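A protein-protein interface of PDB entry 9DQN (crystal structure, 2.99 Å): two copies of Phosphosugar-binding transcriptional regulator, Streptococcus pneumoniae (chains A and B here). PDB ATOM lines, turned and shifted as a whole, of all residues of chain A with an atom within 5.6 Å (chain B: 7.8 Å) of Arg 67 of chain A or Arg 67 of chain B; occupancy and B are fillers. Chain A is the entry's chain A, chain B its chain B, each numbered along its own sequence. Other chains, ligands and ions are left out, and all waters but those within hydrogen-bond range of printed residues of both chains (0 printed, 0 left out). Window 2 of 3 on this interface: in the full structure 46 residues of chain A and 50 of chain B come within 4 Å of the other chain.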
ATOM      1  N   GLY A  65     -34.952  -5.006 -10.267  1.00  0.00           N
ATOM      2  CA  GLY A  65     -34.785  -5.722  -9.020  1.00  0.00           C
ATOM      3  C   GLY A  65     -34.647  -4.767  -7.856  1.00  0.00           C
ATOM      4  O   GLY A  65     -34.811  -3.553  -7.996  1.00  0.00           O
ATOM      5  N   TYR A  66     -34.343  -5.347  -6.692  1.00  0.00           N
ATOM      6  CA  TYR A  66     -34.236  -4.564  -5.466  1.00  0.00           C
ATOM      7  C   TYR A  66     -33.093  -3.559  -5.534  1.00  0.00           C
ATOM      8  O   TYR A  66     -33.172  -2.490  -4.918  1.00  0.00           O
ATOM      9  CB  TYR A  66     -34.059  -5.509  -4.275  1.00  0.00           C
ATOM     10  CG  TYR A  66     -34.037  -4.847  -2.917  1.00  0.00           C
ATOM     11  CD1 TYR A  66     -35.209  -4.394  -2.323  1.00  0.00           C
ATOM     12  CD2 TYR A  66     -32.849  -4.706  -2.214  1.00  0.00           C
ATOM     13  CE1 TYR A  66     -35.192  -3.801  -1.074  1.00  0.00           C
ATOM     14  CE2 TYR A  66     -32.823  -4.117  -0.967  1.00  0.00           C
ATOM     15  CZ  TYR A  66     -33.994  -3.668  -0.402  1.00  0.00           C
ATOM     16  OH  TYR A  66     -33.964  -3.078   0.838  1.00  0.00           O
ATOM     17  N   ARG A  67     -32.029  -3.880  -6.276  1.00  0.00           N
ATOM     18  CA  ARG A  67     -30.897  -2.964  -6.382  1.00  0.00           C
ATOM     19  C   ARG A  67     -31.297  -1.656  -7.054  1.00  0.00           C
ATOM     20  O   ARG A  67     -30.913  -0.573  -6.596  1.00  0.00           O
ATOM     21  CB  ARG A  67     -29.750  -3.623  -7.144  1.00  0.00           C
ATOM     22  CG  ARG A  67     -28.826  -4.456  -6.276  1.00  0.00           C
ATOM     23  CD  ARG A  67     -27.500  -4.690  -6.977  1.00  0.00           C
ATOM     24  NE  ARG A  67     -26.636  -5.595  -6.231  1.00  0.00           N
ATOM     25  CZ  ARG A  67     -26.582  -6.905  -6.427  1.00  0.00           C
ATOM     26  NH1 ARG A  67     -27.338  -7.499  -7.338  1.00  0.00           N
ATOM     27  NH2 ARG A  67     -25.750  -7.638  -5.693  1.00  0.00           N
ATOM     28  N   GLU A  68     -32.063  -1.733  -8.145  1.00  0.00           N
ATOM     29  CA  GLU A  68     -32.493  -0.511  -8.815  1.00  0.00           C
ATOM     30  C   GLU A  68     -33.490   0.270  -7.970  1.00  0.00           C
ATOM     31  O   GLU A  68     -33.503   1.505  -8.015  1.00  0.00           O
ATOM     32  CB  GLU A  68     -33.096  -0.833 -10.183  1.00  0.00           C
ATOM     33  CG  GLU A  68     -33.413   0.404 -11.015  1.00  0.00           C
ATOM     34  CD  GLU A  68     -34.162   0.078 -12.292  1.00  0.00           C
ATOM     35  OE1 GLU A  68     -34.302  -1.121 -12.608  1.00  0.00           O
ATOM     36  OE2 GLU A  68     -34.611   1.022 -12.978  1.00  0.00           O
ATOM     37  N   PHE A  69     -34.330  -0.424  -7.198  1.00  0.00           N
ATOM     38  CA  PHE A  69     -35.320   0.265  -6.379  1.00  0.00           C
ATOM     39  C   PHE A  69     -34.655   1.120  -5.304  1.00  0.00           C
ATOM     40  O   PHE A  69     -34.995   2.298  -5.140  1.00  0.00           O
ATOM     41  CB  PHE A  69     -36.283  -0.745  -5.750  1.00  0.00           C
ATOM     42  CG  PHE A  69     -37.207  -0.141  -4.728  1.00  0.00           C
ATOM     43  CD1 PHE A  69     -38.270   0.655  -5.116  1.00  0.00           C
ATOM     44  CD2 PHE A  69     -37.009  -0.370  -3.379  1.00  0.00           C
ATOM     45  CE1 PHE A  69     -39.116   1.213  -4.175  1.00  0.00           C
ATOM     46  CE2 PHE A  69     -37.849   0.186  -2.434  1.00  0.00           C
ATOM     47  CZ  PHE A  69     -38.905   0.978  -2.832  1.00  0.00           C
ATOM     48  N   ILE A  70     -33.699   0.547  -4.566  1.00  0.00           N
ATOM     49  CA  ILE A  70     -33.029   1.300  -3.505  1.00  0.00           C
ATOM     50  C   ILE A  70     -32.269   2.481  -4.090  1.00  0.00           C
ATOM     51  O   ILE A  70     -32.303   3.592  -3.547  1.00  0.00           O
ATOM     52  CB  ILE A  70     -32.108   0.376  -2.682  1.00  0.00           C
ATOM     53  CG1 ILE A  70     -32.807  -0.074  -1.400  1.00  0.00           C
ATOM     54  CG2 ILE A  70     -30.819   1.087  -2.292  1.00  0.00           C
ATOM     55  CD1 ILE A  70     -34.152  -0.696  -1.623  1.00  0.00           C
ATOM     56  N   PHE A  71     -31.574   2.262  -5.209  1.00  0.00           N
ATOM     57  CA  PHE A  71     -30.836   3.352  -5.836  1.00  0.00           C
ATOM     58  C   PHE A  71     -31.778   4.447  -6.317  1.00  0.00           C
ATOM     59  O   PHE A  71     -31.495   5.636  -6.141  1.00  0.00           O
ATOM     60  CB  PHE A  71     -29.974   2.810  -6.976  1.00  0.00           C
ATOM     61  CG  PHE A  71     -28.814   1.972  -6.505  1.00  0.00           C
ATOM     62  CD1 PHE A  71     -28.373   2.058  -5.194  1.00  0.00           C
ATOM     63  CD2 PHE A  71     -28.166   1.105  -7.366  1.00  0.00           C
ATOM     64  CE1 PHE A  71     -27.309   1.293  -4.753  1.00  0.00           C
ATOM     65  CE2 PHE A  71     -27.101   0.336  -6.933  1.00  0.00           C
ATOM     66  CZ  PHE A  71     -26.671   0.432  -5.624  1.00  0.00           C
ATOM     67  N   GLN A  72     -32.914   4.070  -6.908  1.00  0.00           N
ATOM     68  CA  GLN A  72     -33.939   5.062  -7.220  1.00  0.00           C
ATOM     69  C   GLN A  72     -34.498   5.686  -5.946  1.00  0.00           C
ATOM     70  O   GLN A  72     -34.780   6.890  -5.906  1.00  0.00           O
ATOM     71  CB  GLN A  72     -35.059   4.424  -8.046  1.00  0.00           C
ATOM     72  CG  GLN A  72     -36.137   5.401  -8.506  1.00  0.00           C
ATOM     73  CD  GLN A  72     -35.664   6.322  -9.617  1.00  0.00           C
ATOM     74  OE1 GLN A  72     -34.663   6.051 -10.280  1.00  0.00           O
ATOM     75  NE2 GLN A  72     -36.386   7.418  -9.825  1.00  0.00           N
ATOM     76  N   SER B  40     -22.443  -5.136 -18.227  1.00  0.00           N
ATOM     77  CA  SER B  40     -21.008  -5.340 -18.046  1.00  0.00           C
ATOM     78  C   SER B  40     -20.468  -6.380 -19.019  1.00  0.00           C
ATOM     79  O   SER B  40     -19.348  -6.245 -19.523  1.00  0.00           O
ATOM     80  CB  SER B  40     -20.714  -5.751 -16.605  1.00  0.00           C
ATOM     81  OG  SER B  40     -19.354  -6.109 -16.432  1.00  0.00           O
ATOM     82  N   LEU B  54     -14.497  -2.240 -15.167  1.00  0.00           N
ATOM     83  CA  LEU B  54     -15.687  -1.397 -15.094  1.00  0.00           C
ATOM     84  C   LEU B  54     -16.001  -1.004 -13.656  1.00  0.00           C
ATOM     85  O   LEU B  54     -16.371   0.145 -13.384  1.00  0.00           O
ATOM     86  CB  LEU B  54     -16.879  -2.119 -15.721  1.00  0.00           C
ATOM     87  CG  LEU B  54     -16.854  -2.299 -17.237  1.00  0.00           C
ATOM     88  CD1 LEU B  54     -18.009  -3.179 -17.683  1.00  0.00           C
ATOM     89  CD2 LEU B  54     -16.908  -0.948 -17.929  1.00  0.00           C
ATOM     90  N   THR B  55     -15.872  -1.950 -12.722  1.00  0.00           N
ATOM     91  CA  THR B  55     -16.100  -1.633 -11.315  1.00  0.00           C
ATOM     92  C   THR B  55     -15.085  -0.615 -10.808  1.00  0.00           C
ATOM     93  O   THR B  55     -15.447   0.336 -10.105  1.00  0.00           O
ATOM     94  CB  THR B  55     -16.044  -2.910 -10.473  1.00  0.00           C
ATOM     95  OG1 THR B  55     -17.061  -3.820 -10.912  1.00  0.00           O
ATOM     96  CG2 THR B  55     -16.261  -2.591  -9.002  1.00  0.00           C
ATOM     97  N   ALA B  58     -15.893   2.861 -12.179  1.00  0.00           N
ATOM     98  CA  ALA B  58     -17.024   3.465 -11.485  1.00  0.00           C
ATOM     99  C   ALA B  58     -16.641   3.904 -10.077  1.00  0.00           C
ATOM    100  O   ALA B  58     -17.121   4.937  -9.594  1.00  0.00           O
ATOM    101  CB  ALA B  58     -18.194   2.485 -11.447  1.00  0.00           C
ATOM    102  N   PHE B  63     -18.705   6.050  -7.143  1.00  0.00           N
ATOM    103  CA  PHE B  63     -19.836   5.137  -7.094  1.00  0.00           C
ATOM    104  C   PHE B  63     -19.443   3.858  -6.365  1.00  0.00           C
ATOM    105  O   PHE B  63     -18.261   3.521  -6.249  1.00  0.00           O
ATOM    106  CB  PHE B  63     -20.342   4.800  -8.506  1.00  0.00           C
ATOM    107  CG  PHE B  63     -20.926   5.975  -9.241  1.00  0.00           C
ATOM    108  CD1 PHE B  63     -20.108   6.865  -9.918  1.00  0.00           C
ATOM    109  CD2 PHE B  63     -22.295   6.185  -9.259  1.00  0.00           C
ATOM    110  CE1 PHE B  63     -20.644   7.945 -10.596  1.00  0.00           C
ATOM    111  CE2 PHE B  63     -22.837   7.264  -9.937  1.00  0.00           C
ATOM    112  CZ  PHE B  63     -22.011   8.144 -10.606  1.00  0.00           C
ATOM    113  N   THR B  64     -20.457   3.152  -5.863  1.00  0.00           N
ATOM    114  CA  THR B  64     -20.216   1.864  -5.220  1.00  0.00           C
ATOM    115  C   THR B  64     -19.674   0.845  -6.216  1.00  0.00           C
ATOM    116  O   THR B  64     -18.795   0.044  -5.879  1.00  0.00           O
ATOM    117  CB  THR B  64     -21.502   1.350  -4.572  1.00  0.00           C
ATOM    118  OG1 THR B  64     -22.460   1.038  -5.591  1.00  0.00           O
ATOM    119  CG2 THR B  64     -22.085   2.404  -3.644  1.00  0.00           C
ATOM    120  N   GLY B  65     -20.185   0.861  -7.439  1.00  0.00           N
ATOM    121  CA  GLY B  65     -19.711  -0.053  -8.456  1.00  0.00           C
ATOM    122  C   GLY B  65     -20.281   0.303  -9.810  1.00  0.00           C
ATOM    123  O   GLY B  65     -20.917   1.344  -9.984  1.00  0.00           O
ATOM    124  N   TYR B  66     -20.037  -0.584 -10.779  1.00  0.00           N
ATOM    125  CA  TYR B  66     -20.535  -0.345 -12.129  1.00  0.00           C
ATOM    126  C   TYR B  66     -22.055  -0.357 -12.178  1.00  0.00           C
ATOM    127  O   TYR B  66     -22.655   0.362 -12.985  1.00  0.00           O
ATOM    128  CB  TYR B  66     -19.968  -1.381 -13.099  1.00  0.00           C
ATOM    129  CG  TYR B  66     -20.455  -1.206 -14.520  1.00  0.00           C
ATOM    130  CD1 TYR B  66     -19.938  -0.206 -15.334  1.00  0.00           C
ATOM    131  CD2 TYR B  66     -21.432  -2.040 -15.048  1.00  0.00           C
ATOM    132  CE1 TYR B  66     -20.382  -0.040 -16.633  1.00  0.00           C
ATOM    133  CE2 TYR B  66     -21.881  -1.882 -16.344  1.00  0.00           C
ATOM    134  CZ  TYR B  66     -21.353  -0.882 -17.133  1.00  0.00           C
ATOM    135  OH  TYR B  66     -21.800  -0.726 -18.425  1.00  0.00           O
ATOM    136  N   ARG B  67     -22.696  -1.168 -11.332  1.00  0.00           N
ATOM    137  CA  ARG B  67     -24.153  -1.214 -11.322  1.00  0.00           C
ATOM    138  C   ARG B  67     -24.747   0.134 -10.936  1.00  0.00           C
ATOM    139  O   ARG B  67     -25.708   0.597 -11.561  1.00  0.00           O
ATOM    140  CB  ARG B  67     -24.640  -2.315 -10.377  1.00  0.00           C
ATOM    141  CG  ARG B  67     -25.016  -3.612 -11.083  1.00  0.00           C
ATOM    142  CD  ARG B  67     -25.709  -4.586 -10.139  1.00  0.00           C
ATOM    143  NE  ARG B  67     -24.767  -5.340  -9.321  1.00  0.00           N
ATOM    144  CZ  ARG B  67     -24.495  -6.628  -9.488  1.00  0.00           C
ATOM    145  NH1 ARG B  67     -25.090  -7.343 -10.430  1.00  0.00           N
ATOM    146  NH2 ARG B  67     -23.610  -7.215  -8.687  1.00  0.00           N
ATOM    147  N   GLU B  68     -24.185   0.788  -9.916  1.00  0.00           N
ATOM    148  CA  GLU B  68     -24.692   2.099  -9.522  1.00  0.00           C
ATOM    149  C   GLU B  68     -24.343   3.171 -10.546  1.00  0.00           C
ATOM    150  O   GLU B  68     -25.140   4.087 -10.777  1.00  0.00           O
ATOM    151  CB  GLU B  68     -24.159   2.485  -8.140  1.00  0.00           C
ATOM    152  CG  GLU B  68     -24.687   3.819  -7.619  1.00  0.00           C
ATOM    153  CD  GLU B  68     -24.214   4.135  -6.208  1.00  0.00           C
ATOM    154  OE1 GLU B  68     -24.692   3.480  -5.257  1.00  0.00           O
ATOM    155  OE2 GLU B  68     -23.362   5.036  -6.053  1.00  0.00           O
ATOM    156  N   PHE B  69     -23.163   3.079 -11.167  1.00  0.00           N
ATOM    157  CA  PHE B  69     -22.786   4.060 -12.182  1.00  0.00           C
ATOM    158  C   PHE B  69     -23.725   4.000 -13.380  1.00  0.00           C
ATOM    159  O   PHE B  69     -24.250   5.028 -13.825  1.00  0.00           O
ATOM    160  CB  PHE B  69     -21.340   3.835 -12.626  1.00  0.00           C
ATOM    161  CG  PHE B  69     -20.975   4.570 -13.887  1.00  0.00           C
ATOM    162  CD1 PHE B  69     -20.680   5.922 -13.855  1.00  0.00           C
ATOM    163  CD2 PHE B  69     -20.939   3.909 -15.107  1.00  0.00           C
ATOM    164  CE1 PHE B  69     -20.353   6.603 -15.012  1.00  0.00           C
ATOM    165  CE2 PHE B  69     -20.614   4.585 -16.268  1.00  0.00           C
ATOM    166  CZ  PHE B  69     -20.319   5.933 -16.220  1.00  0.00           C
ATOM    167  N   ILE B  70     -23.955   2.795 -13.911  1.00  0.00           N
ATOM    168  CA  ILE B  70     -24.802   2.641 -15.087  1.00  0.00           C
ATOM    169  C   ILE B  70     -26.243   3.029 -14.789  1.00  0.00           C
ATOM    170  O   ILE B  70     -26.995   3.369 -15.709  1.00  0.00           O
ATOM    171  CB  ILE B  70     -24.710   1.195 -15.626  1.00  0.00           C
ATOM    172  CG1 ILE B  70     -25.015   1.162 -17.123  1.00  0.00           C
ATOM    173  CG2 ILE B  70     -25.647   0.264 -14.871  1.00  0.00           C
ATOM    174  CD1 ILE B  70     -23.955   1.837 -17.964  1.00  0.00           C
ATOM    175  N   PHE B  71     -26.649   2.992 -13.518  1.00  0.00           N
ATOM    176  CA  PHE B  71     -28.002   3.409 -13.170  1.00  0.00           C
ATOM    177  C   PHE B  71     -28.152   4.920 -13.280  1.00  0.00           C
ATOM    178  O   PHE B  71     -29.129   5.412 -13.854  1.00  0.00           O
ATOM    179  CB  PHE B  71     -28.362   2.920 -11.768  1.00  0.00           C
ATOM    180  CG  PHE B  71     -28.651   1.445 -11.700  1.00  0.00           C
ATOM    181  CD1 PHE B  71     -28.760   0.689 -12.857  1.00  0.00           C
ATOM    182  CD2 PHE B  71     -28.819   0.816 -10.481  1.00  0.00           C
ATOM    183  CE1 PHE B  71     -29.028  -0.668 -12.795  1.00  0.00           C
ATOM    184  CE2 PHE B  71     -29.086  -0.539 -10.410  1.00  0.00           C
ATOM    185  CZ  PHE B  71     -29.191  -1.282 -11.569  1.00  0.00           C
ATOM    186  N   GLN B  72     -27.186   5.675 -12.749  1.00  0.00           N
ATOM    187  CA  GLN B  72     -27.202   7.124 -12.928  1.00  0.00           C
ATOM    188  C   GLN B  72     -27.080   7.491 -14.401  1.00  0.00           C
ATOM    189  O   GLN B  72     -27.749   8.415 -14.879  1.00  0.00           O
ATOM    190  CB  GLN B  72     -26.073   7.770 -12.120  1.00  0.00           C
ATOM    191  CG  GLN B  72     -26.524   8.841 -11.129  1.00  0.00           C
ATOM    192  CD  GLN B  72     -26.981  10.132 -11.795  1.00  0.00           C
ATOM    193  OE1 GLN B  72     -26.966  10.261 -13.019  1.00  0.00           O
ATOM    194  NE2 GLN B  72     -27.386  11.100 -10.981  1.00  0.00           N
ATOM    195  N   TYR B  73     -26.232   6.772 -15.137  1.00  0.00           N
ATOM    196  CA  TYR B  73     -26.058   7.047 -16.560  1.00  0.00           C
ATOM    197  C   TYR B  73     -27.365   6.845 -17.319  1.00  0.00           C
ATOM    198  O   TYR B  73     -27.740   7.669 -18.162  1.00  0.00           O
ATOM    199  CB  TYR B  73     -24.953   6.153 -17.126  1.00  0.00           C
ATOM    200  CG  TYR B  73     -24.464   6.563 -18.496  1.00  0.00           C
ATOM    201  CD1 TYR B  73     -23.764   7.749 -18.677  1.00  0.00           C
ATOM    202  CD2 TYR B  73     -24.690   5.759 -19.607  1.00  0.00           C
ATOM    203  CE1 TYR B  73     -23.311   8.130 -19.925  1.00  0.00           C
ATOM    204  CE2 TYR B  73     -24.237   6.131 -20.862  1.00  0.00           C
ATOM    205  CZ  TYR B  73     -23.548   7.317 -21.015  1.00  0.00           C
ATOM    206  OH  TYR B  73     -23.097   7.692 -22.260  1.00  0.00           O
ATOM    207  N   GLN B  74     -28.075   5.752 -17.030  1.00  0.00           N
ATOM    208  CA  GLN B  74     -29.359   5.511 -17.678  1.00  0.00           C
ATOM    209  C   GLN B  74     -30.470   6.376 -17.093  1.00  0.00           C
ATOM    210  O   GLN B  74     -31.391   6.765 -17.820  1.00  0.00           O
ATOM    211  CB  GLN B  74     -29.736   4.030 -17.576  1.00  0.00           C
ATOM    212  CG  GLN B  74     -28.950   3.120 -18.510  1.00  0.00           C
ATOM    213  CD  GLN B  74     -29.535   1.722 -18.591  1.00  0.00           C
ATOM    214  OE1 GLN B  74     -30.183   1.251 -17.656  1.00  0.00           O
ATOM    215  NE2 GLN B  74     -29.317   1.054 -19.719  1.00  0.00           N
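OE1 of Glu 68 of chain B sits close to OG1 of Thr 64 of chain B, 3.3 Å away.
Arg 67 of chain A touches Arg 67 of chain B. CE2 of Phe 71 of chain B touches CA of Glu 68 of chain A (3.8 Å). Phe 71 of chain A touches Glu 68 of chain B. Phe 71 of chain A touches Phe 71 of chain B (CD2 to CD2, 3.2 Å).
Arg 67 of chain A touches one residue of chain B. Of chain A, only Arg 67 comes within 4 Å of Arg 67 of chain B. Of the printed residues of chain B, Glu 68 of chain A touches Phe 71 (3.8 Å). Printed residues of chain B within 4 Å of Phe 71 of chain A: Glu 68 (3.4 Å) and Phe 71 (3.2 Å). Of the printed residues of chain A, Phe 71 of chain B touches Glu 68 (3.8 Å) and Phe 71 (3.2 Å). Printed residues of chain A within 4 Å of Glu 68 of chain B: Phe 71 (3.4 Å). The nearest residue of chain A that does not touch Arg 67 of chain B is Phe 71 of chain A (4.6 Å). The nearest printed residue of chain A that does not touch Glu 68 of chain B is Arg 67 of chain A (7.0 Å).
Of the 8 printed residues of chain A, 3 touch a printed residue of chain B. Printed residues of chain B that touch a printed residue of chain A: Arg 67, Glu 68 and Phe 71. Hydrophobic or aromatic side chains of chain B that line the printed part of chain A: Phe 71. Among the printed residues, 4 pairs touch across the chains.
Arg 67 of chain A touches its own counterpart, Arg 67 of chain B. Glu 68 of chain A touches Phe 71 of chain B, and with the chains exchanged Phe 71 of chain A touches Glu 68 of chain B. Phe 71 of chain B touches its own counterpart, Phe 71 of chain A. Of the 4 pairs that touch across the chains among the printed residues, 4 have their exchanged pair printed and touching as well.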
